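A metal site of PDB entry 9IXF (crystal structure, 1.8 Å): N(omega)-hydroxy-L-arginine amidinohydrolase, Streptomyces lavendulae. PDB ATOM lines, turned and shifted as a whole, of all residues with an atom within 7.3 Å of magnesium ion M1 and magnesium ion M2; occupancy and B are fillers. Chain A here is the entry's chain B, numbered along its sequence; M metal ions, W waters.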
ATOM      1  N   MET A  18      27.234   1.888 -14.576  1.00  0.00           N
ATOM      2  CA  MET A  18      26.136   2.039 -15.526  1.00  0.00           C
ATOM      3  C   MET A  18      26.151   0.959 -16.608  1.00  0.00           C
ATOM      4  O   MET A  18      25.087   0.609 -17.145  1.00  0.00           O
ATOM      5  CB  MET A  18      26.151   3.461 -16.119  1.00  0.00           C
ATOM      6  CG  MET A  18      25.391   4.469 -15.202  1.00  0.00           C
ATOM      7  SD  MET A  18      25.550   6.180 -15.717  1.00  0.00           S
ATOM      8  CE  MET A  18      27.290   6.175 -16.011  1.00  0.00           C
ATOM      9  N   THR A  85      24.322   4.769 -20.860  1.00  0.00           N
ATOM     10  CA  THR A  85      24.207   6.217 -20.682  1.00  0.00           C
ATOM     11  C   THR A  85      23.230   6.809 -21.684  1.00  0.00           C
ATOM     12  O   THR A  85      22.990   6.228 -22.739  1.00  0.00           O
ATOM     13  CB  THR A  85      25.562   6.914 -20.853  1.00  0.00           C
ATOM     14  OG1 THR A  85      26.001   6.775 -22.210  1.00  0.00           O
ATOM     15  CG2 THR A  85      26.607   6.329 -19.922  1.00  0.00           C
ATOM     16  N   CYS A  86      22.706   7.991 -21.347  1.00  0.00           N
ATOM     17  CA  CYS A  86      21.887   8.754 -22.297  1.00  0.00           C
ATOM     18  C   CYS A  86      22.641   9.044 -23.587  1.00  0.00           C
ATOM     19  O   CYS A  86      22.025   9.192 -24.639  1.00  0.00           O
ATOM     20  CB  CYS A  86      21.450  10.081 -21.680  1.00  0.00           C
ATOM     21  SG  CYS A  86      20.008  10.003 -20.606  1.00  0.00           S
ATOM     22  N   SER A  87      23.975   9.148 -23.526  1.00  0.00           N
ATOM     23  CA  SER A  87      24.752   9.525 -24.710  1.00  0.00           C
ATOM     24  C   SER A  87      24.637   8.508 -25.830  1.00  0.00           C
ATOM     25  O   SER A  87      24.907   8.842 -26.975  1.00  0.00           O
ATOM     26  CB  SER A  87      26.222   9.717 -24.360  1.00  0.00           C
ATOM     27  OG  SER A  87      26.374  10.745 -23.407  1.00  0.00           O
ATOM     28  N   TYR A 107      11.205  12.673 -24.072  1.00  0.00           N
ATOM     29  CA  TYR A 107      12.529  12.616 -23.464  1.00  0.00           C
ATOM     30  C   TYR A 107      12.293  12.789 -21.972  1.00  0.00           C
ATOM     31  O   TYR A 107      12.164  13.894 -21.470  1.00  0.00           O
ATOM     32  CB  TYR A 107      13.450  13.699 -24.039  1.00  0.00           C
ATOM     33  CG  TYR A 107      14.916  13.419 -23.811  1.00  0.00           C
ATOM     34  CD1 TYR A 107      15.535  13.799 -22.621  1.00  0.00           C
ATOM     35  CD2 TYR A 107      15.676  12.788 -24.782  1.00  0.00           C
ATOM     36  CE1 TYR A 107      16.874  13.547 -22.398  1.00  0.00           C
ATOM     37  CE2 TYR A 107      17.039  12.526 -24.571  1.00  0.00           C
ATOM     38  CZ  TYR A 107      17.626  12.907 -23.377  1.00  0.00           C
ATOM     39  OH  TYR A 107      18.955  12.654 -23.155  1.00  0.00           O
ATOM     40  N   ILE A 108      12.164  11.659 -21.277  1.00  0.00           N
ATOM     41  CA  ILE A 108      11.763  11.668 -19.873  1.00  0.00           C
ATOM     42  C   ILE A 108      13.027  11.679 -19.026  1.00  0.00           C
ATOM     43  O   ILE A 108      13.760  10.689 -18.970  1.00  0.00           O
ATOM     44  CB  ILE A 108      10.869  10.467 -19.543  1.00  0.00           C
ATOM     45  CG1 ILE A 108       9.705  10.393 -20.554  1.00  0.00           C
ATOM     46  CG2 ILE A 108      10.357  10.620 -18.108  1.00  0.00           C
ATOM     47  CD1 ILE A 108       8.683   9.265 -20.298  1.00  0.00           C
ATOM     48  N   ASP A 109      13.306  12.811 -18.382  1.00  0.00           N
ATOM     49  CA  ASP A 109      14.642  13.097 -17.892  1.00  0.00           C
ATOM     50  C   ASP A 109      14.557  14.172 -16.811  1.00  0.00           C
ATOM     51  O   ASP A 109      13.759  15.109 -16.932  1.00  0.00           O
ATOM     52  CB  ASP A 109      15.516  13.571 -19.083  1.00  0.00           C
ATOM     53  CG  ASP A 109      16.999  13.601 -18.776  1.00  0.00           C
ATOM     54  OD1 ASP A 109      17.468  14.626 -18.203  1.00  0.00           O
ATOM     55  OD2 ASP A 109      17.695  12.632 -19.164  1.00  0.00           O
ATOM     56  N   GLY A 110      15.385  14.048 -15.780  1.00  0.00           N
ATOM     57  CA  GLY A 110      15.388  15.053 -14.736  1.00  0.00           C
ATOM     58  C   GLY A 110      16.042  16.370 -15.112  1.00  0.00           C
ATOM     59  O   GLY A 110      15.839  17.370 -14.424  1.00  0.00           O
ATOM     60  N   HIS A 111      16.800  16.403 -16.208  1.00  0.00           N
ATOM     61  CA  HIS A 111      17.650  17.551 -16.516  1.00  0.00           C
ATOM     62  C   HIS A 111      17.311  18.289 -17.796  1.00  0.00           C
ATOM     63  O   HIS A 111      17.359  19.521 -17.818  1.00  0.00           O
ATOM     64  CB  HIS A 111      19.106  17.106 -16.582  1.00  0.00           C
ATOM     65  CG  HIS A 111      19.644  16.662 -15.268  1.00  0.00           C
ATOM     66  ND1 HIS A 111      20.250  17.530 -14.376  1.00  0.00           N
ATOM     67  CD2 HIS A 111      19.652  15.453 -14.670  1.00  0.00           C
ATOM     68  CE1 HIS A 111      20.620  16.862 -13.303  1.00  0.00           C
ATOM     69  NE2 HIS A 111      20.270  15.595 -13.456  1.00  0.00           N
ATOM     70  N   GLY A 112      17.013  17.590 -18.884  1.00  0.00           N
ATOM     71  CA  GLY A 112      16.789  18.205 -20.172  1.00  0.00           C
ATOM     72  C   GLY A 112      17.851  17.875 -21.212  1.00  0.00           C
ATOM     73  O   GLY A 112      17.536  17.795 -22.400  1.00  0.00           O
ATOM     74  N   ASP A 113      19.104  17.688 -20.781  1.00  0.00           N
ATOM     75  CA  ASP A 113      20.198  17.243 -21.652  1.00  0.00           C
ATOM     76  C   ASP A 113      20.241  18.030 -22.955  1.00  0.00           C
ATOM     77  O   ASP A 113      20.409  17.481 -24.053  1.00  0.00           O
ATOM     78  CB  ASP A 113      20.088  15.743 -21.927  1.00  0.00           C
ATOM     79  CG  ASP A 113      20.186  14.926 -20.653  1.00  0.00           C
ATOM     80  OD1 ASP A 113      20.603  15.503 -19.616  1.00  0.00           O
ATOM     81  OD2 ASP A 113      19.877  13.714 -20.707  1.00  0.00           O
ATOM     82  N   TYR A 124      30.020  17.335 -19.774  1.00  0.00           N
ATOM     83  CA  TYR A 124      29.472  15.971 -19.823  1.00  0.00           C
ATOM     84  C   TYR A 124      28.647  15.750 -21.076  1.00  0.00           C
ATOM     85  O   TYR A 124      27.610  16.416 -21.277  1.00  0.00           O
ATOM     86  CB  TYR A 124      28.616  15.715 -18.591  1.00  0.00           C
ATOM     87  CG  TYR A 124      28.054  14.310 -18.536  1.00  0.00           C
ATOM     88  CD1 TYR A 124      28.847  13.212 -18.850  1.00  0.00           C
ATOM     89  CD2 TYR A 124      26.733  14.087 -18.139  1.00  0.00           C
ATOM     90  CE1 TYR A 124      28.335  11.917 -18.785  1.00  0.00           C
ATOM     91  CE2 TYR A 124      26.223  12.785 -18.082  1.00  0.00           C
ATOM     92  CZ  TYR A 124      27.020  11.724 -18.400  1.00  0.00           C
ATOM     93  OH  TYR A 124      26.496  10.441 -18.336  1.00  0.00           O
ATOM     94  N   GLY A 126      26.646  13.434 -21.701  1.00  0.00           N
ATOM     95  CA  GLY A 126      25.300  12.993 -21.374  1.00  0.00           C
ATOM     96  C   GLY A 126      24.320  14.117 -21.164  1.00  0.00           C
ATOM     97  O   GLY A 126      23.107  13.883 -21.183  1.00  0.00           O
ATOM     98  N   GLY A 127      24.805  15.343 -20.964  1.00  0.00           N
ATOM     99  CA  GLY A 127      23.962  16.517 -20.873  1.00  0.00           C
ATOM    100  C   GLY A 127      23.815  17.276 -22.175  1.00  0.00           C
ATOM    101  O   GLY A 127      23.269  18.384 -22.163  1.00  0.00           O
ATOM    102  N   VAL A 129      22.672  15.501 -25.163  1.00  0.00           N
ATOM    103  CA  VAL A 129      22.124  14.478 -26.050  1.00  0.00           C
ATOM    104  C   VAL A 129      20.953  15.016 -26.875  1.00  0.00           C
ATOM    105  O   VAL A 129      20.914  14.843 -28.097  1.00  0.00           O
ATOM    106  CB  VAL A 129      21.681  13.252 -25.228  1.00  0.00           C
ATOM    107  CG1 VAL A 129      20.984  12.225 -26.151  1.00  0.00           C
ATOM    108  CG2 VAL A 129      22.878  12.645 -24.538  1.00  0.00           C
ATOM    109  N   HIS A 196      12.203   7.875 -24.426  1.00  0.00           N
ATOM    110  CA  HIS A 196      13.551   7.831 -23.880  1.00  0.00           C
ATOM    111  C   HIS A 196      13.440   8.121 -22.404  1.00  0.00           C
ATOM    112  O   HIS A 196      12.906   9.163 -22.025  1.00  0.00           O
ATOM    113  CB  HIS A 196      14.422   8.880 -24.589  1.00  0.00           C
ATOM    114  CG  HIS A 196      15.789   9.039 -23.988  1.00  0.00           C
ATOM    115  ND1 HIS A 196      16.928   8.596 -24.612  1.00  0.00           N
ATOM    116  CD2 HIS A 196      16.189   9.647 -22.844  1.00  0.00           C
ATOM    117  CE1 HIS A 196      17.980   8.881 -23.866  1.00  0.00           C
ATOM    118  NE2 HIS A 196      17.563   9.521 -22.783  1.00  0.00           N
ATOM    119  N   ILE A 197      13.897   7.208 -21.541  1.00  0.00           N
ATOM    120  CA  ILE A 197      13.819   7.512 -20.111  1.00  0.00           C
ATOM    121  C   ILE A 197      15.180   7.365 -19.426  1.00  0.00           C
ATOM    122  O   ILE A 197      15.869   6.345 -19.575  1.00  0.00           O
ATOM    123  CB  ILE A 197      12.735   6.683 -19.399  1.00  0.00           C
ATOM    124  CG1 ILE A 197      12.562   7.163 -17.949  1.00  0.00           C
ATOM    125  CG2 ILE A 197      13.019   5.205 -19.490  1.00  0.00           C
ATOM    126  CD1 ILE A 197      11.133   6.865 -17.389  1.00  0.00           C
ATOM    127  N   ASP A 198      15.575   8.430 -18.702  1.00  0.00           N
ATOM    128  CA  ASP A 198      16.723   8.490 -17.808  1.00  0.00           C
ATOM    129  C   ASP A 198      16.184   8.401 -16.379  1.00  0.00           C
ATOM    130  O   ASP A 198      15.393   9.259 -15.970  1.00  0.00           O
ATOM    131  CB  ASP A 198      17.464   9.811 -18.054  1.00  0.00           C
ATOM    132  CG  ASP A 198      18.710  10.027 -17.193  1.00  0.00           C
ATOM    133  OD1 ASP A 198      18.901   9.399 -16.136  1.00  0.00           O
ATOM    134  OD2 ASP A 198      19.529  10.900 -17.602  1.00  0.00           O
ATOM    135  N   TRP A 199      16.583   7.366 -15.627  1.00  0.00           N
ATOM    136  CA  TRP A 199      16.009   7.187 -14.292  1.00  0.00           C
ATOM    137  C   TRP A 199      16.269   8.342 -13.328  1.00  0.00           C
ATOM    138  O   TRP A 199      15.625   8.374 -12.261  1.00  0.00           O
ATOM    139  CB  TRP A 199      16.503   5.871 -13.671  1.00  0.00           C
ATOM    140  CG  TRP A 199      16.184   4.718 -14.569  1.00  0.00           C
ATOM    141  CD1 TRP A 199      17.075   3.846 -15.132  1.00  0.00           C
ATOM    142  CD2 TRP A 199      14.895   4.339 -15.059  1.00  0.00           C
ATOM    143  NE1 TRP A 199      16.416   2.945 -15.939  1.00  0.00           N
ATOM    144  CE2 TRP A 199      15.075   3.225 -15.911  1.00  0.00           C
ATOM    145  CE3 TRP A 199      13.589   4.837 -14.861  1.00  0.00           C
ATOM    146  CZ2 TRP A 199      14.021   2.592 -16.546  1.00  0.00           C
ATOM    147  CZ3 TRP A 199      12.537   4.204 -15.510  1.00  0.00           C
ATOM    148  CH2 TRP A 199      12.764   3.105 -16.350  1.00  0.00           C
ATOM    149  N   ASP A 200      17.146   9.295 -13.657  1.00  0.00           N
ATOM    150  CA  ASP A 200      17.252  10.454 -12.780  1.00  0.00           C
ATOM    151  C   ASP A 200      15.988  11.310 -12.803  1.00  0.00           C
ATOM    152  O   ASP A 200      15.885  12.246 -11.987  1.00  0.00           O
ATOM    153  CB  ASP A 200      18.518  11.283 -13.097  1.00  0.00           C
ATOM    154  CG  ASP A 200      18.519  11.956 -14.488  1.00  0.00           C
ATOM    155  OD1 ASP A 200      17.449  12.358 -14.983  1.00  0.00           O
ATOM    156  OD2 ASP A 200      19.626  12.131 -15.079  1.00  0.00           O
ATOM    157  N   VAL A 201      15.030  11.032 -13.682  1.00  0.00           N
ATOM    158  CA  VAL A 201      13.757  11.742 -13.656  1.00  0.00           C
ATOM    159  C   VAL A 201      12.991  11.464 -12.366  1.00  0.00           C
ATOM    160  O   VAL A 201      12.180  12.304 -11.931  1.00  0.00           O
ATOM    161  CB  VAL A 201      12.903  11.385 -14.890  1.00  0.00           C
ATOM    162  CG1 VAL A 201      12.367   9.969 -14.777  1.00  0.00           C
ATOM    163  CG2 VAL A 201      11.752  12.374 -15.045  1.00  0.00           C
ATOM    164  N   ALA A 209      20.941   6.367  -9.386  1.00  0.00           N
ATOM    165  CA  ALA A 209      21.428   7.015 -10.594  1.00  0.00           C
ATOM    166  C   ALA A 209      22.320   8.172 -10.178  1.00  0.00           C
ATOM    167  O   ALA A 209      22.218   8.681  -9.054  1.00  0.00           O
ATOM    168  CB  ALA A 209      20.261   7.504 -11.471  1.00  0.00           C
ATOM    169  N   ASP A 210      23.215   8.576 -11.079  1.00  0.00           N
ATOM    170  CA  ASP A 210      23.996   9.768 -10.823  1.00  0.00           C
ATOM    171  C   ASP A 210      23.209  11.003 -11.256  1.00  0.00           C
ATOM    172  O   ASP A 210      22.235  10.913 -12.006  1.00  0.00           O
ATOM    173  CB  ASP A 210      25.353   9.697 -11.536  1.00  0.00           C
ATOM    174  CG  ASP A 210      25.225   9.632 -13.060  1.00  0.00           C
ATOM    175  OD1 ASP A 210      24.148   9.220 -13.558  1.00  0.00           O
ATOM    176  OD2 ASP A 210      26.210   9.982 -13.762  1.00  0.00           O
ATOM    177  N   TYR A 211      23.621  12.164 -10.754  1.00  0.00           N
ATOM    178  CA  TYR A 211      22.958  13.433 -11.060  1.00  0.00           C
ATOM    179  C   TYR A 211      21.499  13.435 -10.616  1.00  0.00           C
ATOM    180  O   TYR A 211      20.609  13.884 -11.339  1.00  0.00           O
ATOM    181  CB  TYR A 211      23.055  13.752 -12.557  1.00  0.00           C
ATOM    182  CG  TYR A 211      24.449  13.943 -13.098  1.00  0.00           C
ATOM    183  CD1 TYR A 211      25.143  15.126 -12.872  1.00  0.00           C
ATOM    184  CD2 TYR A 211      25.075  12.964 -13.856  1.00  0.00           C
ATOM    185  CE1 TYR A 211      26.419  15.322 -13.367  1.00  0.00           C
ATOM    186  CE2 TYR A 211      26.355  13.139 -14.359  1.00  0.00           C
ATOM    187  CZ  TYR A 211      27.016  14.324 -14.115  1.00  0.00           C
ATOM    188  OH  TYR A 211      28.289  14.534 -14.610  1.00  0.00           O
ATOM    189  N   THR A 212      21.236  12.913  -9.408  1.00  0.00           N
ATOM    190  CA  THR A 212      19.884  12.982  -8.844  1.00  0.00           C
ATOM    191  C   THR A 212      19.488  14.435  -8.623  1.00  0.00           C
ATOM    192  O   THR A 212      20.355  15.306  -8.438  1.00  0.00           O
ATOM    193  CB  THR A 212      19.809  12.196  -7.523  1.00  0.00           C
ATOM    194  OG1 THR A 212      20.558  12.871  -6.512  1.00  0.00           O
ATOM    195  CG2 THR A 212      20.363  10.800  -7.697  1.00  0.00           C
ATOM    196  N   ALA A 240      17.667   4.042 -19.645  1.00  0.00           N
ATOM    197  CA  ALA A 240      19.065   4.391 -19.445  1.00  0.00           C
ATOM    198  C   ALA A 240      19.371   4.837 -18.027  1.00  0.00           C
ATOM    199  O   ALA A 240      18.543   5.465 -17.362  1.00  0.00           O
ATOM    200  CB  ALA A 240      19.489   5.517 -20.401  1.00  0.00           C
ATOM    201  N   GLU A 241      20.597   4.508 -17.584  1.00  0.00           N
ATOM    202  CA  GLU A 241      21.355   5.153 -16.502  1.00  0.00           C
ATOM    203  C   GLU A 241      21.043   4.617 -15.115  1.00  0.00           C
ATOM    204  O   GLU A 241      21.141   5.347 -14.124  1.00  0.00           O
ATOM    205  CB  GLU A 241      21.168   6.680 -16.541  1.00  0.00           C
ATOM    206  CG  GLU A 241      21.601   7.251 -17.886  1.00  0.00           C
ATOM    207  CD  GLU A 241      22.296   8.568 -17.796  1.00  0.00           C
ATOM    208  OE1 GLU A 241      23.081   8.860 -18.720  1.00  0.00           O
ATOM    209  OE2 GLU A 241      22.065   9.318 -16.816  1.00  0.00           O
HETATM  210 MG    MG M   1      19.735  12.236 -19.240  1.00  0.00          MG
HETATM  211 MG    MG M   2      20.838  10.650 -15.895  1.00  0.00          MG
HETATM  212  O   HOH W   1      21.587   9.836 -14.129  1.00  0.00           O
HETATM  213  O   HOH W   2      21.804  12.109 -19.265  1.00  0.00           O
HETATM  214  O   HOH W   3      19.973  13.569 -17.616  1.00  0.00           O
HETATM  215  O   HOH W   4      22.251  12.003 -16.265  1.00  0.00           O
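The side-chain carboxylate of Glu 241 is in hydrogen-bond range of the backbone NH of Cys 86 (2.8 Å).
N of His 111 is in hydrogen-bond range of OD1 of Asp 109 (2.8 Å).
OD1 of Asp 109 sits at hydrogen-bond distance from N of Gly 112 (3.1 Å).
OD1 of Asp 200 sits at hydrogen-bond distance from N of Gly 110 (2.8 Å).
The side-chain hydroxyl of Tyr 107 lies close to the side-chain carboxylate of Asp 113 (2.8 Å).
The backbone carbonyl oxygen of Asp 113 sits at hydrogen-bond distance from the backbone NH of Val 129, at 3.2 Å.
The backbone carbonyl oxygen (O) of Ile 108 sits at hydrogen-bond distance from the backbone NH (N) of Asp 198, at 2.9 Å.
A ring nitrogen (NE2) of His 196 lies close to the side-chain sulfur (SG) of Cys 86, at 3.3 Å.
Four residues have an atom within 4 Å of magnesium ion M1: Cys 86, Asp 109, Asp 113 and Asp 198.
Within 4 Å of magnesium ion M2: Asp 198, Asp 200 and Glu 241.
Magnesium ion M1 is bound by water W2, the side-chain carboxylate (OD2) of Asp 109, the side-chain carboxylate (OD2) of Asp 113, water W3, the side-chain carboxylate (OD2) of Asp 198 and the side-chain sulfur (SG) of Cys 86.
Magnesium ion M1 has six donor atoms within binding distance.
Magnesium ion M2 is bound by water W4, OE2 of Glu 241, OD2 of Asp 200, water W1, OD2 of Asp 198 and OD1 of Asp 198.
Water W3 lies within hydrogen-bond range of the side-chain carboxylate (OD1) of Asp 109 (2.8 Å) and the side-chain carboxylate (OD1) of Asp 113 (2.9 Å).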
